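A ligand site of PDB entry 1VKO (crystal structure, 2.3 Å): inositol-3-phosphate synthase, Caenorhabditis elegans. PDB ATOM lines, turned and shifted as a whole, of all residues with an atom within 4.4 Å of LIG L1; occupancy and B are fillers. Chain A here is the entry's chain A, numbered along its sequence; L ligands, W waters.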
ATOM      1  N   VAL A  82     -11.565  23.746  -3.404  1.00  0.00           N
ATOM      2  CA  VAL A  82     -11.694  23.142  -4.721  1.00  0.00           C
ATOM      3  C   VAL A  82     -11.452  21.670  -4.554  1.00  0.00           C
ATOM      4  O   VAL A  82     -10.445  21.242  -3.954  1.00  0.00           O
ATOM      5  CB  VAL A  82     -10.772  23.758  -5.750  1.00  0.00           C
ATOM      6  CG1 VAL A  82     -11.187  23.334  -7.150  1.00  0.00           C
ATOM      7  CG2 VAL A  82     -10.786  25.296  -5.602  1.00  0.00           C
ATOM      8  N   GLY A  83     -12.389  20.874  -5.059  1.00  0.00           N
ATOM      9  CA  GLY A  83     -12.439  19.459  -4.729  1.00  0.00           C
ATOM     10  C   GLY A  83     -13.198  19.286  -3.415  1.00  0.00           C
ATOM     11  O   GLY A  83     -12.820  18.482  -2.592  1.00  0.00           O
ATOM     12  N   GLY A  85     -15.882  17.854  -2.722  1.00  0.00           N
ATOM     13  CA  GLY A  85     -16.515  16.545  -2.591  1.00  0.00           C
ATOM     14  C   GLY A  85     -15.571  15.386  -2.529  1.00  0.00           C
ATOM     15  O   GLY A  85     -16.011  14.234  -2.539  1.00  0.00           O
ATOM     16  N   GLY A  86     -14.268  15.658  -2.446  1.00  0.00           N
ATOM     17  CA  GLY A  86     -13.235  14.588  -2.417  1.00  0.00           C
ATOM     18  C   GLY A  86     -13.105  13.917  -1.068  1.00  0.00           C
ATOM     19  O   GLY A  86     -13.931  14.150  -0.168  1.00  0.00           O
ATOM     20  N   ASN A  87     -12.082  13.067  -0.917  1.00  0.00           N
ATOM     21  CA  ASN A  87     -11.797  12.467   0.384  1.00  0.00           C
ATOM     22  C   ASN A  87     -11.457  13.537   1.423  1.00  0.00           C
ATOM     23  O   ASN A  87     -12.101  13.582   2.458  1.00  0.00           O
ATOM     24  CB  ASN A  87     -10.672  11.412   0.343  1.00  0.00           C
ATOM     25  CG  ASN A  87     -11.106  10.118  -0.283  1.00  0.00           C
ATOM     26  OD1 ASN A  87     -12.007  10.082  -1.134  1.00  0.00           O
ATOM     27  ND2 ASN A  87     -10.461   9.035   0.121  1.00  0.00           N
ATOM     28  N   ASN A  88     -10.437  14.360   1.138  1.00  0.00           N
ATOM     29  CA  ASN A  88     -10.050  15.442   2.079  1.00  0.00           C
ATOM     30  C   ASN A  88     -11.207  16.410   2.306  1.00  0.00           C
ATOM     31  O   ASN A  88     -11.596  16.682   3.443  1.00  0.00           O
ATOM     32  CB  ASN A  88      -8.790  16.174   1.603  1.00  0.00           C
ATOM     33  CG  ASN A  88      -7.579  15.219   1.502  1.00  0.00           C
ATOM     34  OD1 ASN A  88      -7.603  14.159   2.103  1.00  0.00           O
ATOM     35  ND2 ASN A  88      -6.531  15.591   0.745  1.00  0.00           N
ATOM     36  N   TRP A 159     -16.235  23.879  -4.561  1.00  0.00           N
ATOM     37  CA  TRP A 159     -16.615  23.378  -5.875  1.00  0.00           C
ATOM     38  C   TRP A 159     -16.208  21.940  -6.143  1.00  0.00           C
ATOM     39  O   TRP A 159     -15.193  21.466  -5.635  1.00  0.00           O
ATOM     40  CB  TRP A 159     -15.987  24.216  -6.949  1.00  0.00           C
ATOM     41  CG  TRP A 159     -16.238  25.685  -6.871  1.00  0.00           C
ATOM     42  CD1 TRP A 159     -17.194  26.399  -7.526  1.00  0.00           C
ATOM     43  CD2 TRP A 159     -15.455  26.640  -6.141  1.00  0.00           C
ATOM     44  NE1 TRP A 159     -17.078  27.735  -7.230  1.00  0.00           N
ATOM     45  CE2 TRP A 159     -16.024  27.913  -6.380  1.00  0.00           C
ATOM     46  CE3 TRP A 159     -14.346  26.548  -5.286  1.00  0.00           C
ATOM     47  CZ2 TRP A 159     -15.494  29.087  -5.809  1.00  0.00           C
ATOM     48  CZ3 TRP A 159     -13.807  27.693  -4.758  1.00  0.00           C
ATOM     49  CH2 TRP A 159     -14.389  28.961  -5.008  1.00  0.00           C
ATOM     50  N   ASP A 160     -16.962  21.261  -6.982  1.00  0.00           N
ATOM     51  CA  ASP A 160     -16.541  19.954  -7.398  1.00  0.00           C
ATOM     52  C   ASP A 160     -17.113  19.588  -8.747  1.00  0.00           C
ATOM     53  O   ASP A 160     -18.278  19.816  -8.971  1.00  0.00           O
ATOM     54  CB  ASP A 160     -16.925  18.897  -6.388  1.00  0.00           C
ATOM     55  CG  ASP A 160     -15.936  17.728  -6.356  1.00  0.00           C
ATOM     56  OD1 ASP A 160     -15.713  17.090  -7.388  1.00  0.00           O
ATOM     57  OD2 ASP A 160     -15.305  17.387  -5.338  1.00  0.00           O
ATOM     58  N   ILE A 161     -16.268  19.034  -9.623  1.00  0.00           N
ATOM     59  CA  ILE A 161     -16.729  18.509 -10.914  1.00  0.00           C
ATOM     60  C   ILE A 161     -17.753  17.360 -10.743  1.00  0.00           C
ATOM     61  O   ILE A 161     -18.466  17.016 -11.683  1.00  0.00           O
ATOM     62  CB  ILE A 161     -15.552  18.077 -11.810  1.00  0.00           C
ATOM     63  CG1 ILE A 161     -14.787  16.905 -11.175  1.00  0.00           C
ATOM     64  CG2 ILE A 161     -14.623  19.284 -12.098  1.00  0.00           C
ATOM     65  CD1 ILE A 161     -13.687  16.225 -12.084  1.00  0.00           C
ATOM     66  N   SER A 162     -17.830  16.790  -9.546  1.00  0.00           N
ATOM     67  CA  SER A 162     -18.834  15.751  -9.233  1.00  0.00           C
ATOM     68  C   SER A 162     -19.960  16.332  -8.398  1.00  0.00           C
ATOM     69  O   SER A 162     -19.701  16.985  -7.378  1.00  0.00           O
ATOM     70  CB  SER A 162     -18.211  14.609  -8.442  1.00  0.00           C
ATOM     71  OG  SER A 162     -19.250  13.683  -8.126  1.00  0.00           O
ATOM     72  N   SER A 196     -17.675  23.192 -11.241  1.00  0.00           N
ATOM     73  CA  SER A 196     -16.340  23.730 -11.367  1.00  0.00           C
ATOM     74  C   SER A 196     -15.883  23.801 -12.807  1.00  0.00           C
ATOM     75  O   SER A 196     -16.591  23.396 -13.727  1.00  0.00           O
ATOM     76  CB  SER A 196     -15.330  22.879 -10.585  1.00  0.00           C
ATOM     77  OG  SER A 196     -14.296  23.708 -10.080  1.00  0.00           O
ATOM     78  N   ILE A 197     -14.664  24.300 -12.975  1.00  0.00           N
ATOM     79  CA  ILE A 197     -13.987  24.364 -14.264  1.00  0.00           C
ATOM     80  C   ILE A 197     -13.445  22.965 -14.439  1.00  0.00           C
ATOM     81  O   ILE A 197     -12.858  22.429 -13.515  1.00  0.00           O
ATOM     82  CB  ILE A 197     -12.841  25.373 -14.147  1.00  0.00           C
ATOM     83  CG1 ILE A 197     -13.390  26.733 -13.750  1.00  0.00           C
ATOM     84  CG2 ILE A 197     -12.053  25.501 -15.438  1.00  0.00           C
ATOM     85  CD1 ILE A 197     -12.310  27.708 -13.391  1.00  0.00           C
ATOM     86  N   ILE A 203      -5.754  16.873 -15.903  1.00  0.00           N
ATOM     87  CA  ILE A 203      -5.691  15.779 -14.887  1.00  0.00           C
ATOM     88  C   ILE A 203      -5.678  14.387 -15.517  1.00  0.00           C
ATOM     89  O   ILE A 203      -5.670  14.298 -16.755  1.00  0.00           O
ATOM     90  CB  ILE A 203      -6.863  15.865 -13.857  1.00  0.00           C
ATOM     91  CG1 ILE A 203      -8.183  15.487 -14.488  1.00  0.00           C
ATOM     92  CG2 ILE A 203      -6.972  17.264 -13.255  1.00  0.00           C
ATOM     93  CD1 ILE A 203      -9.382  16.010 -13.729  1.00  0.00           C
ATOM     94  N   ARG A 210     -16.473  10.894 -13.838  1.00  0.00           N
ATOM     95  CA  ARG A 210     -16.851  11.529 -12.575  1.00  0.00           C
ATOM     96  C   ARG A 210     -17.369  12.970 -12.773  1.00  0.00           C
ATOM     97  O   ARG A 210     -18.041  13.523 -11.897  1.00  0.00           O
ATOM     98  CB  ARG A 210     -15.663  11.504 -11.611  1.00  0.00           C
ATOM     99  CG  ARG A 210     -15.855  12.178 -10.251  1.00  0.00           C
ATOM    100  CD  ARG A 210     -14.551  12.479  -9.538  1.00  0.00           C
ATOM    101  NE  ARG A 210     -14.228  11.418  -8.585  1.00  0.00           N
ATOM    102  CZ  ARG A 210     -14.559  11.418  -7.306  1.00  0.00           C
ATOM    103  NH1 ARG A 210     -15.235  12.451  -6.784  1.00  0.00           N
ATOM    104  NH2 ARG A 210     -14.212  10.391  -6.536  1.00  0.00           N
ATOM    105  N   TRP A 247      -7.045  24.693  -2.745  1.00  0.00           N
ATOM    106  CA  TRP A 247      -7.084  23.620  -3.694  1.00  0.00           C
ATOM    107  C   TRP A 247      -6.772  22.262  -3.037  1.00  0.00           C
ATOM    108  O   TRP A 247      -5.635  21.985  -2.581  1.00  0.00           O
ATOM    109  CB  TRP A 247      -6.095  23.893  -4.831  1.00  0.00           C
ATOM    110  CG  TRP A 247      -6.129  22.828  -5.874  1.00  0.00           C
ATOM    111  CD1 TRP A 247      -5.574  21.582  -5.804  1.00  0.00           C
ATOM    112  CD2 TRP A 247      -6.779  22.901  -7.144  1.00  0.00           C
ATOM    113  NE1 TRP A 247      -5.842  20.875  -6.949  1.00  0.00           N
ATOM    114  CE2 TRP A 247      -6.587  21.654  -7.799  1.00  0.00           C
ATOM    115  CE3 TRP A 247      -7.533  23.899  -7.810  1.00  0.00           C
ATOM    116  CZ2 TRP A 247      -7.082  21.389  -9.080  1.00  0.00           C
ATOM    117  CZ3 TRP A 247      -8.064  23.618  -9.049  1.00  0.00           C
ATOM    118  CH2 TRP A 247      -7.817  22.375  -9.687  1.00  0.00           C
ATOM    119  N   THR A 248      -7.776  21.406  -3.053  1.00  0.00           N
ATOM    120  CA  THR A 248      -7.656  20.038  -2.610  1.00  0.00           C
ATOM    121  C   THR A 248      -8.452  19.127  -3.568  1.00  0.00           C
ATOM    122  O   THR A 248      -9.072  18.141  -3.156  1.00  0.00           O
ATOM    123  CB  THR A 248      -8.097  19.860  -1.113  1.00  0.00           C
ATOM    124  OG1 THR A 248      -7.994  18.481  -0.757  1.00  0.00           O
ATOM    125  CG2 THR A 248      -9.618  20.188  -0.873  1.00  0.00           C
ATOM    126  N   ALA A 249      -8.437  19.501  -4.848  1.00  0.00           N
ATOM    127  CA  ALA A 249      -8.901  18.658  -5.951  1.00  0.00           C
ATOM    128  C   ALA A 249      -7.741  17.844  -6.584  1.00  0.00           C
ATOM    129  O   ALA A 249      -6.631  17.893  -6.128  1.00  0.00           O
ATOM    130  CB  ALA A 249      -9.574  19.543  -7.008  1.00  0.00           C
ATOM    131  N   ASN A 250      -8.010  17.070  -7.623  1.00  0.00           N
ATOM    132  CA  ASN A 250      -6.997  16.188  -8.156  1.00  0.00           C
ATOM    133  C   ASN A 250      -5.782  16.929  -8.665  1.00  0.00           C
ATOM    134  O   ASN A 250      -5.862  18.057  -9.154  1.00  0.00           O
ATOM    135  CB  ASN A 250      -7.539  15.254  -9.228  1.00  0.00           C
ATOM    136  CG  ASN A 250      -8.522  14.252  -8.648  1.00  0.00           C
ATOM    137  OD1 ASN A 250      -9.737  14.469  -8.677  1.00  0.00           O
ATOM    138  ND2 ASN A 250      -7.985  13.195  -7.998  1.00  0.00           N
ATOM    139  N   THR A 251      -4.638  16.282  -8.458  1.00  0.00           N
ATOM    140  CA  THR A 251      -3.383  16.755  -8.927  1.00  0.00           C
ATOM    141  C   THR A 251      -3.526  16.980 -10.410  1.00  0.00           C
ATOM    142  O   THR A 251      -3.846  16.040 -11.139  1.00  0.00           O
ATOM    143  CB  THR A 251      -2.391  15.635  -8.622  1.00  0.00           C
ATOM    144  OG1 THR A 251      -2.235  15.593  -7.215  1.00  0.00           O
ATOM    145  CG2 THR A 251      -0.983  15.978  -9.114  1.00  0.00           C
ATOM    146  N   PRO A 281      -7.095  25.132 -14.848  1.00  0.00           N
ATOM    147  CA  PRO A 281      -8.214  25.377 -13.940  1.00  0.00           C
ATOM    148  C   PRO A 281      -7.709  25.944 -12.608  1.00  0.00           C
ATOM    149  O   PRO A 281      -8.355  26.836 -12.032  1.00  0.00           O
ATOM    150  CB  PRO A 281      -8.761  23.976 -13.714  1.00  0.00           C
ATOM    151  CG  PRO A 281      -8.504  23.303 -15.050  1.00  0.00           C
ATOM    152  CD  PRO A 281      -7.124  23.731 -15.359  1.00  0.00           C
ATOM    153  N   GLY A 299      -2.784  22.899  -2.186  1.00  0.00           N
ATOM    154  CA  GLY A 299      -2.570  21.679  -1.436  1.00  0.00           C
ATOM    155  C   GLY A 299      -2.027  20.548  -2.296  1.00  0.00           C
ATOM    156  O   GLY A 299      -1.712  19.459  -1.779  1.00  0.00           O
ATOM    157  N   SER A 300      -1.878  20.803  -3.591  1.00  0.00           N
ATOM    158  CA  SER A 300      -1.460  19.781  -4.547  1.00  0.00           C
ATOM    159  C   SER A 300      -0.095  20.135  -5.178  1.00  0.00           C
ATOM    160  O   SER A 300       0.433  21.238  -4.973  1.00  0.00           O
ATOM    161  CB  SER A 300      -2.515  19.595  -5.634  1.00  0.00           C
ATOM    162  OG  SER A 300      -3.735  19.134  -5.090  1.00  0.00           O
ATOM    163  N   PRO A 301       0.501  19.157  -5.852  1.00  0.00           N
ATOM    164  CA  PRO A 301       1.811  19.309  -6.452  1.00  0.00           C
ATOM    165  C   PRO A 301       1.919  20.283  -7.628  1.00  0.00           C
ATOM    166  O   PRO A 301       3.027  20.743  -7.870  1.00  0.00           O
ATOM    167  CB  PRO A 301       2.128  17.895  -6.968  1.00  0.00           C
ATOM    168  CG  PRO A 301       1.326  17.029  -6.159  1.00  0.00           C
ATOM    169  CD  PRO A 301       0.006  17.782  -5.997  1.00  0.00           C
ATOM    170  N   ASP A 324       1.551  21.463  -1.724  1.00  0.00           N
ATOM    171  CA  ASP A 324       1.360  20.016  -1.537  1.00  0.00           C
ATOM    172  C   ASP A 324       1.456  19.609  -0.059  1.00  0.00           C
ATOM    173  O   ASP A 324       2.540  19.708   0.556  1.00  0.00           O
ATOM    174  CB  ASP A 324       2.360  19.236  -2.405  1.00  0.00           C
ATOM    175  CG  ASP A 324       1.946  17.788  -2.671  1.00  0.00           C
ATOM    176  OD1 ASP A 324       0.741  17.436  -2.539  1.00  0.00           O
ATOM    177  OD2 ASP A 324       2.760  16.934  -3.072  1.00  0.00           O
ATOM    178  N   PHE A 325       0.317  19.143   0.484  1.00  0.00           N
ATOM    179  CA  PHE A 325       0.236  18.744   1.880  1.00  0.00           C
ATOM    180  C   PHE A 325       1.360  17.865   2.221  1.00  0.00           C
ATOM    181  O   PHE A 325       1.714  16.927   1.473  1.00  0.00           O
ATOM    182  CB  PHE A 325      -1.054  17.981   2.209  1.00  0.00           C
ATOM    183  CG  PHE A 325      -2.341  18.708   1.877  1.00  0.00           C
ATOM    184  CD1 PHE A 325      -2.581  19.993   2.348  1.00  0.00           C
ATOM    185  CD2 PHE A 325      -3.318  18.089   1.119  1.00  0.00           C
ATOM    186  CE1 PHE A 325      -3.801  20.656   2.039  1.00  0.00           C
ATOM    187  CE2 PHE A 325      -4.536  18.762   0.813  1.00  0.00           C
ATOM    188  CZ  PHE A 325      -4.740  20.019   1.280  1.00  0.00           C
ATOM    189  N   SER A 327       1.764  15.375   4.678  1.00  0.00           N
ATOM    190  CA  SER A 327       0.894  14.662   5.613  1.00  0.00           C
ATOM    191  C   SER A 327       1.548  13.429   6.305  1.00  0.00           C
ATOM    192  O   SER A 327       1.328  13.215   7.516  1.00  0.00           O
ATOM    193  CB  SER A 327      -0.413  14.266   4.899  1.00  0.00           C
ATOM    194  OG  SER A 327      -0.181  13.488   3.733  1.00  0.00           O
ATOM    195  N   ASN A 358      -7.421   5.065  -3.061  1.00  0.00           N
ATOM    196  CA  ASN A 358      -8.432   6.126  -3.075  1.00  0.00           C
ATOM    197  C   ASN A 358      -8.471   6.819  -4.449  1.00  0.00           C
ATOM    198  O   ASN A 358      -7.750   6.365  -5.360  1.00  0.00           O
ATOM    199  CB  ASN A 358      -8.292   7.082  -1.860  1.00  0.00           C
ATOM    200  CG  ASN A 358      -6.924   7.766  -1.735  1.00  0.00           C
ATOM    201  OD1 ASN A 358      -6.099   7.776  -2.656  1.00  0.00           O
ATOM    202  ND2 ASN A 358      -6.681   8.340  -0.560  1.00  0.00           N
ATOM    203  N   ASN A 359      -9.299   7.856  -4.632  1.00  0.00           N
ATOM    204  CA  ASN A 359      -9.304   8.596  -5.909  1.00  0.00           C
ATOM    205  C   ASN A 359      -8.028   9.393  -6.170  1.00  0.00           C
ATOM    206  O   ASN A 359      -7.714   9.700  -7.329  1.00  0.00           O
ATOM    207  CB  ASN A 359     -10.505   9.522  -6.085  1.00  0.00           C
ATOM    208  CG  ASN A 359     -10.657  10.017  -7.536  1.00  0.00           C
ATOM    209  OD1 ASN A 359     -10.695   9.215  -8.464  1.00  0.00           O
ATOM    210  ND2 ASN A 359     -10.728  11.344  -7.722  1.00  0.00           N
ATOM    211  N   ASP A 360      -7.321   9.736  -5.092  1.00  0.00           N
ATOM    212  CA  ASP A 360      -6.007  10.372  -5.180  1.00  0.00           C
ATOM    213  C   ASP A 360      -5.031   9.430  -5.931  1.00  0.00           C
ATOM    214  O   ASP A 360      -4.393   9.849  -6.909  1.00  0.00           O
ATOM    215  CB  ASP A 360      -5.498  10.808  -3.777  1.00  0.00           C
ATOM    216  CG  ASP A 360      -4.138  11.541  -3.794  1.00  0.00           C
ATOM    217  OD1 ASP A 360      -3.783  12.159  -4.849  1.00  0.00           O
ATOM    218  OD2 ASP A 360      -3.344  11.535  -2.817  1.00  0.00           O
ATOM    219  N   LYS A 373       3.712  15.140  -8.304  1.00  0.00           N
ATOM    220  CA  LYS A 373       3.960  14.584  -6.951  1.00  0.00           C
ATOM    221  C   LYS A 373       5.390  14.060  -6.672  1.00  0.00           C
ATOM    222  O   LYS A 373       5.965  14.373  -5.619  1.00  0.00           O
ATOM    223  CB  LYS A 373       2.928  13.501  -6.649  1.00  0.00           C
ATOM    224  CG  LYS A 373       2.998  12.979  -5.230  1.00  0.00           C
ATOM    225  CD  LYS A 373       2.324  13.926  -4.215  1.00  0.00           C
ATOM    226  CE  LYS A 373       0.803  13.961  -4.388  1.00  0.00           C
ATOM    227  NZ  LYS A 373       0.286  15.057  -3.533  1.00  0.00           N
ATOM    228  N   ASP A 440      -4.615   8.667   4.881  1.00  0.00           N
ATOM    229  CA  ASP A 440      -4.308   9.961   4.241  1.00  0.00           C
ATOM    230  C   ASP A 440      -5.275  11.095   4.600  1.00  0.00           C
ATOM    231  O   ASP A 440      -4.845  12.189   4.953  1.00  0.00           O
ATOM    232  CB  ASP A 440      -4.266   9.808   2.720  1.00  0.00           C
ATOM    233  CG  ASP A 440      -2.955   9.224   2.245  1.00  0.00           C
ATOM    234  OD1 ASP A 440      -1.903   9.353   2.950  1.00  0.00           O
ATOM    235  OD2 ASP A 440      -2.891   8.614   1.158  1.00  0.00           O
ATOM    236  N   ALA A 444      -4.494  14.511   6.217  1.00  0.00           N
ATOM    237  CA  ALA A 444      -4.619  15.740   5.384  1.00  0.00           C
ATOM    238  C   ALA A 444      -5.513  16.842   5.894  1.00  0.00           C
ATOM    239  O   ALA A 444      -5.111  18.021   5.842  1.00  0.00           O
ATOM    240  CB  ALA A 444      -5.056  15.371   3.996  1.00  0.00           C
ATOM    241  N   LYS A 484       4.960  20.218   1.397  1.00  0.00           N
ATOM    242  CA  LYS A 484       6.054  19.383   0.935  1.00  0.00           C
ATOM    243  C   LYS A 484       7.048  20.143   0.140  1.00  0.00           C
ATOM    244  O   LYS A 484       8.266  19.903   0.268  1.00  0.00           O
ATOM    245  CB  LYS A 484       5.555  18.313  -0.009  1.00  0.00           C
ATOM    246  CG  LYS A 484       5.172  17.039   0.647  1.00  0.00           C
ATOM    247  CD  LYS A 484       5.152  15.931  -0.403  1.00  0.00           C
ATOM    248  CE  LYS A 484       4.210  14.852   0.060  1.00  0.00           C
ATOM    249  NZ  LYS A 484       2.767  15.276  -0.038  1.00  0.00           N
HETATM  250  P1  LIG L   1      -9.969  12.902  -4.076  1.00  0.00           P
HETATM  251  O1  LIG L   1     -10.085  12.319  -5.398  1.00  0.00           O
HETATM  252  O2  LIG L   1     -10.758  12.095  -3.131  1.00  0.00           O
HETATM  253  O3  LIG L   1     -10.450  14.412  -4.179  1.00  0.00           O
HETATM  254  C1  LIG L   1     -10.417  15.076  -5.412  1.00  0.00           C
HETATM  255  C2  LIG L   1     -11.779  15.703  -5.620  1.00  0.00           C
HETATM  256  O4  LIG L   1     -11.623  16.854  -6.419  1.00  0.00           O
HETATM  257  C3  LIG L   1     -12.720  14.801  -6.354  1.00  0.00           C
HETATM  258  O5  LIG L   1     -13.997  15.069  -5.782  1.00  0.00           O
HETATM  259  C4  LIG L   1     -12.789  15.319  -7.765  1.00  0.00           C
HETATM  260  O6  LIG L   1     -14.175  15.274  -8.099  1.00  0.00           O
HETATM  261  C5  LIG L   1     -12.398  16.776  -7.578  1.00  0.00           C
HETATM  262  N1  LIG L   1     -11.813  17.537  -8.717  1.00  0.00           N
HETATM  263  C6  LIG L   1     -10.951  17.139  -9.690  1.00  0.00           C
HETATM  264  N2  LIG L   1     -10.721  18.187 -10.513  1.00  0.00           N
HETATM  265  C7  LIG L   1     -11.422  19.265 -10.111  1.00  0.00           C
HETATM  266  C8  LIG L   1     -11.590  20.572 -10.601  1.00  0.00           C
HETATM  267  N3  LIG L   1     -11.030  21.007 -11.745  1.00  0.00           N
HETATM  268  N4  LIG L   1     -12.430  21.431  -9.939  1.00  0.00           N
HETATM  269  C9  LIG L   1     -13.116  21.010  -8.828  1.00  0.00           C
HETATM  270  N5  LIG L   1     -12.976  19.728  -8.399  1.00  0.00           N
HETATM  271  C10 LIG L   1     -12.137  18.860  -9.001  1.00  0.00           C
HETATM  272  O7  LIG L   1      -8.432  13.042  -3.599  1.00  0.00           O
HETATM  273  P2  LIG L   1      -8.088  13.517  -2.119  1.00  0.00           P
HETATM  274  O8  LIG L   1      -9.245  14.304  -1.634  1.00  0.00           O
HETATM  275  O9  LIG L   1      -7.674  12.321  -1.363  1.00  0.00           O
HETATM  276  O10 LIG L   1      -6.894  14.601  -2.259  1.00  0.00           O
HETATM  277  C11 LIG L   1      -6.982  15.658  -3.210  1.00  0.00           C
HETATM  278  C12 LIG L   1      -5.621  16.264  -3.592  1.00  0.00           C
HETATM  279  O11 LIG L   1      -4.853  16.531  -2.452  1.00  0.00           O
HETATM  280  C13 LIG L   1      -4.765  15.373  -4.492  1.00  0.00           C
HETATM  281  O12 LIG L   1      -4.145  16.168  -5.464  1.00  0.00           O
HETATM  282  C14 LIG L   1      -3.645  14.928  -3.582  1.00  0.00           C
HETATM  283  O13 LIG L   1      -2.395  14.699  -4.223  1.00  0.00           O
HETATM  284  C15 LIG L   1      -3.525  16.131  -2.683  1.00  0.00           C
HETATM  285  N6  LIG L   1      -2.784  15.667  -1.518  1.00  0.00           N
HETATM  286  C16 LIG L   1      -3.294  14.693  -0.719  1.00  0.00           C
HETATM  287  C17 LIG L   1      -2.555  14.249   0.356  1.00  0.00           C
HETATM  288  C18 LIG L   1      -3.312  13.492   1.390  1.00  0.00           C
HETATM  289  O14 LIG L   1      -4.667  13.223   1.068  1.00  0.00           O
HETATM  290  N7  LIG L   1      -2.706  13.131   2.522  1.00  0.00           N
HETATM  291  C19 LIG L   1      -1.299  14.803   0.652  1.00  0.00           C
HETATM  292  C20 LIG L   1      -0.786  15.767  -0.183  1.00  0.00           C
HETATM  293  C21 LIG L   1      -1.540  16.201  -1.282  1.00  0.00           C
HETATM  294  P1  LG2 L   2       3.171  12.172   2.267  1.00  0.00           P
HETATM  295  O1  LG2 L   2       3.452  13.091   3.441  1.00  0.00           O
HETATM  296  O2  LG2 L   2       2.610  10.858   2.760  1.00  0.00           O
HETATM  297  O3  LG2 L   2       4.467  11.894   1.517  1.00  0.00           O
HETATM  298  O4  LG2 L   2       2.045  12.859   1.304  1.00  0.00           O
HETATM  299  P2  LG2 L   2       1.411  12.237  -0.075  1.00  0.00           P
HETATM  300  O5  LG2 L   2       0.055  11.643   0.268  1.00  0.00           O
HETATM  301  O6  LG2 L   2       1.308  13.353  -1.100  1.00  0.00           O
HETATM  302  O7  LG2 L   2       2.215  11.102  -0.723  1.00  0.00           O
HETATM  303  O   HOH W   1      -4.872  10.323  -0.482  1.00  0.00           O
HETATM  304  O   HOH W   2     -11.036  16.760  -1.776  1.00  0.00           O
HETATM  305  O   HOH W   3      -8.149  20.384 -12.823  1.00  0.00           O
HETATM  306  O   HOH W   4      -9.070   9.884  -2.592  1.00  0.00           O
HETATM  307  O   HOH W   5      -4.779  13.427  -7.011  1.00  0.00           O
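Val 82 touches LIG L1.
Gly 83 touches LIG L1.
Gly 85 touches LIG L1.
Trp 159 touches LIG L1.
Ile 161 touches LIG L1.
Thr 248 touches LIG L1.
Gly 299 touches LIG L1 (O to C21, 3.3 Å).
OD1 of Asp 324 touches C21 of LIG L1 (2.9 Å).
Phe 325 touches LIG L1.
CB of Ala 444 touches N7 of LIG L1, at 3.6 Å.
NZ of Lys 484 touches C20 of LIG L1 (3.6 Å).
Of the 33 residues printed, 27 come within 4 Å of LIG L1.
Water W2 lies within hydrogen-bond range of O of Gly 83 (2.6 Å), O of Thr 248 (2.8 Å), O8 of LIG L1 (3.0 Å) and N of Gly 86 (3.5 Å).
Water W5 lies within hydrogen-bond range of OD1 of Asp 360 (2.7 Å), N of Thr 251 (3.2 Å), O12 of LIG L1 (3.2 Å) and ND2 of Asn 250 (3.4 Å).
The side-chain amide nitrogen of Asn 250 sits close to the side-chain amide nitrogen of Asn 359, 3.3 Å away.
N of Asp 324 sits at hydrogen-bond distance from O of Ser 300 (3.4 Å).
OG of Ser 300 is in hydrogen-bond range of O of Ala 249.
The backbone carbonyl oxygen (O) of Ala 249 sits at hydrogen-bond distance from the indole nitrogen (NE1) of Trp 247 (3.2 Å).
The side-chain amino group (NZ) of Lys 484 is in salt-bridge range of the side-chain carboxylate (OD2) of Asp 324 (3.5 Å).
The side-chain carboxylate (OD1) of Asp 324 lies within salt-bridge range of the side-chain amino group (NZ) of Lys 373, at 2.6 Å.
N of Phe 325 lies within hydrogen-bond range of O of Gly 299 (3.1 Å).
The side-chain carboxylate of Asp 160 lies close to the backbone NH of Ser 162, at 3.0 Å.
OG of Ser 327 sits at hydrogen-bond distance from N7 of LIG L1, at 2.8 Å.
O of Asp 440 sits at hydrogen-bond distance from N7 of LIG L1, 3.4 Å away.
The backbone NH (N) of Asn 88 lies within hydrogen-bond range of an oxygen (O8) of LIG L1.
NZ of Lys 373 is in salt-bridge range of O6 of LG2 L2, 3.1 Å away.
OG of Ser 300 lies within hydrogen-bond range of O12 of LIG L1 (3.0 Å).
OG1 of Thr 251 lies within hydrogen-bond range of O12 of LIG L1, at 2.7 Å.
An oxygen (O12) of LIG L1 sits at hydrogen-bond distance from the backbone NH (N) of Thr 251, at 3.0 Å.
An oxygen (O5) of LIG L1 sits at hydrogen-bond distance from the backbone NH (N) of Gly 86 (3.4 Å).
O1 of LG2 L2 lies within hydrogen-bond range of N of Ser 327 (3.1 Å).
OD1 of Asp 360 sits at hydrogen-bond distance from O13 of LIG L1 (3.0 Å).
The side-chain hydroxyl (OG) of Ser 196 is in hydrogen-bond range of a nitrogen (N4) of LIG L1.
An oxygen (O12) of LIG L1 sits at hydrogen-bond distance from the backbone carbonyl oxygen (O) of Ala 249, at 3.1 Å.
NH1 of Arg 210 sits at hydrogen-bond distance from O5 of LIG L1.
ND2 of Asn 359 lies within hydrogen-bond range of O1 of LIG L1.
O13 of LIG L1 is in hydrogen-bond range of NZ of Lys 373 (2.8 Å).
OG of Ser 327 lies within hydrogen-bond range of O4 of LG2 L2 (3.4 Å).
The side-chain amide oxygen (OD1) of Asn 87 lies close to an oxygen (O2) of LIG L1 (3.1 Å).
The side-chain amide nitrogen (ND2) of Asn 250 is in hydrogen-bond range of an oxygen (O1) of LIG L1 (3.5 Å).
The backbone carbonyl oxygen (O) of Ile 197 is in hydrogen-bond range of a nitrogen (N3) of LIG L1, 2.9 Å away.
The backbone NH (N) of Asn 87 lies within hydrogen-bond range of an oxygen (O2) of LIG L1.
The side-chain amide nitrogen (ND2) of Asn 88 is in hydrogen-bond range of an oxygen (O14) of LIG L1, at 3.0 Å.
NZ of Lys 484 is in salt-bridge range of O6 of LG2 L2 (2.6 Å).
An oxygen (O6) of LIG L1 sits at hydrogen-bond distance from the side-chain carboxylate (OD1) of Asp 160, at 2.5 Å.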
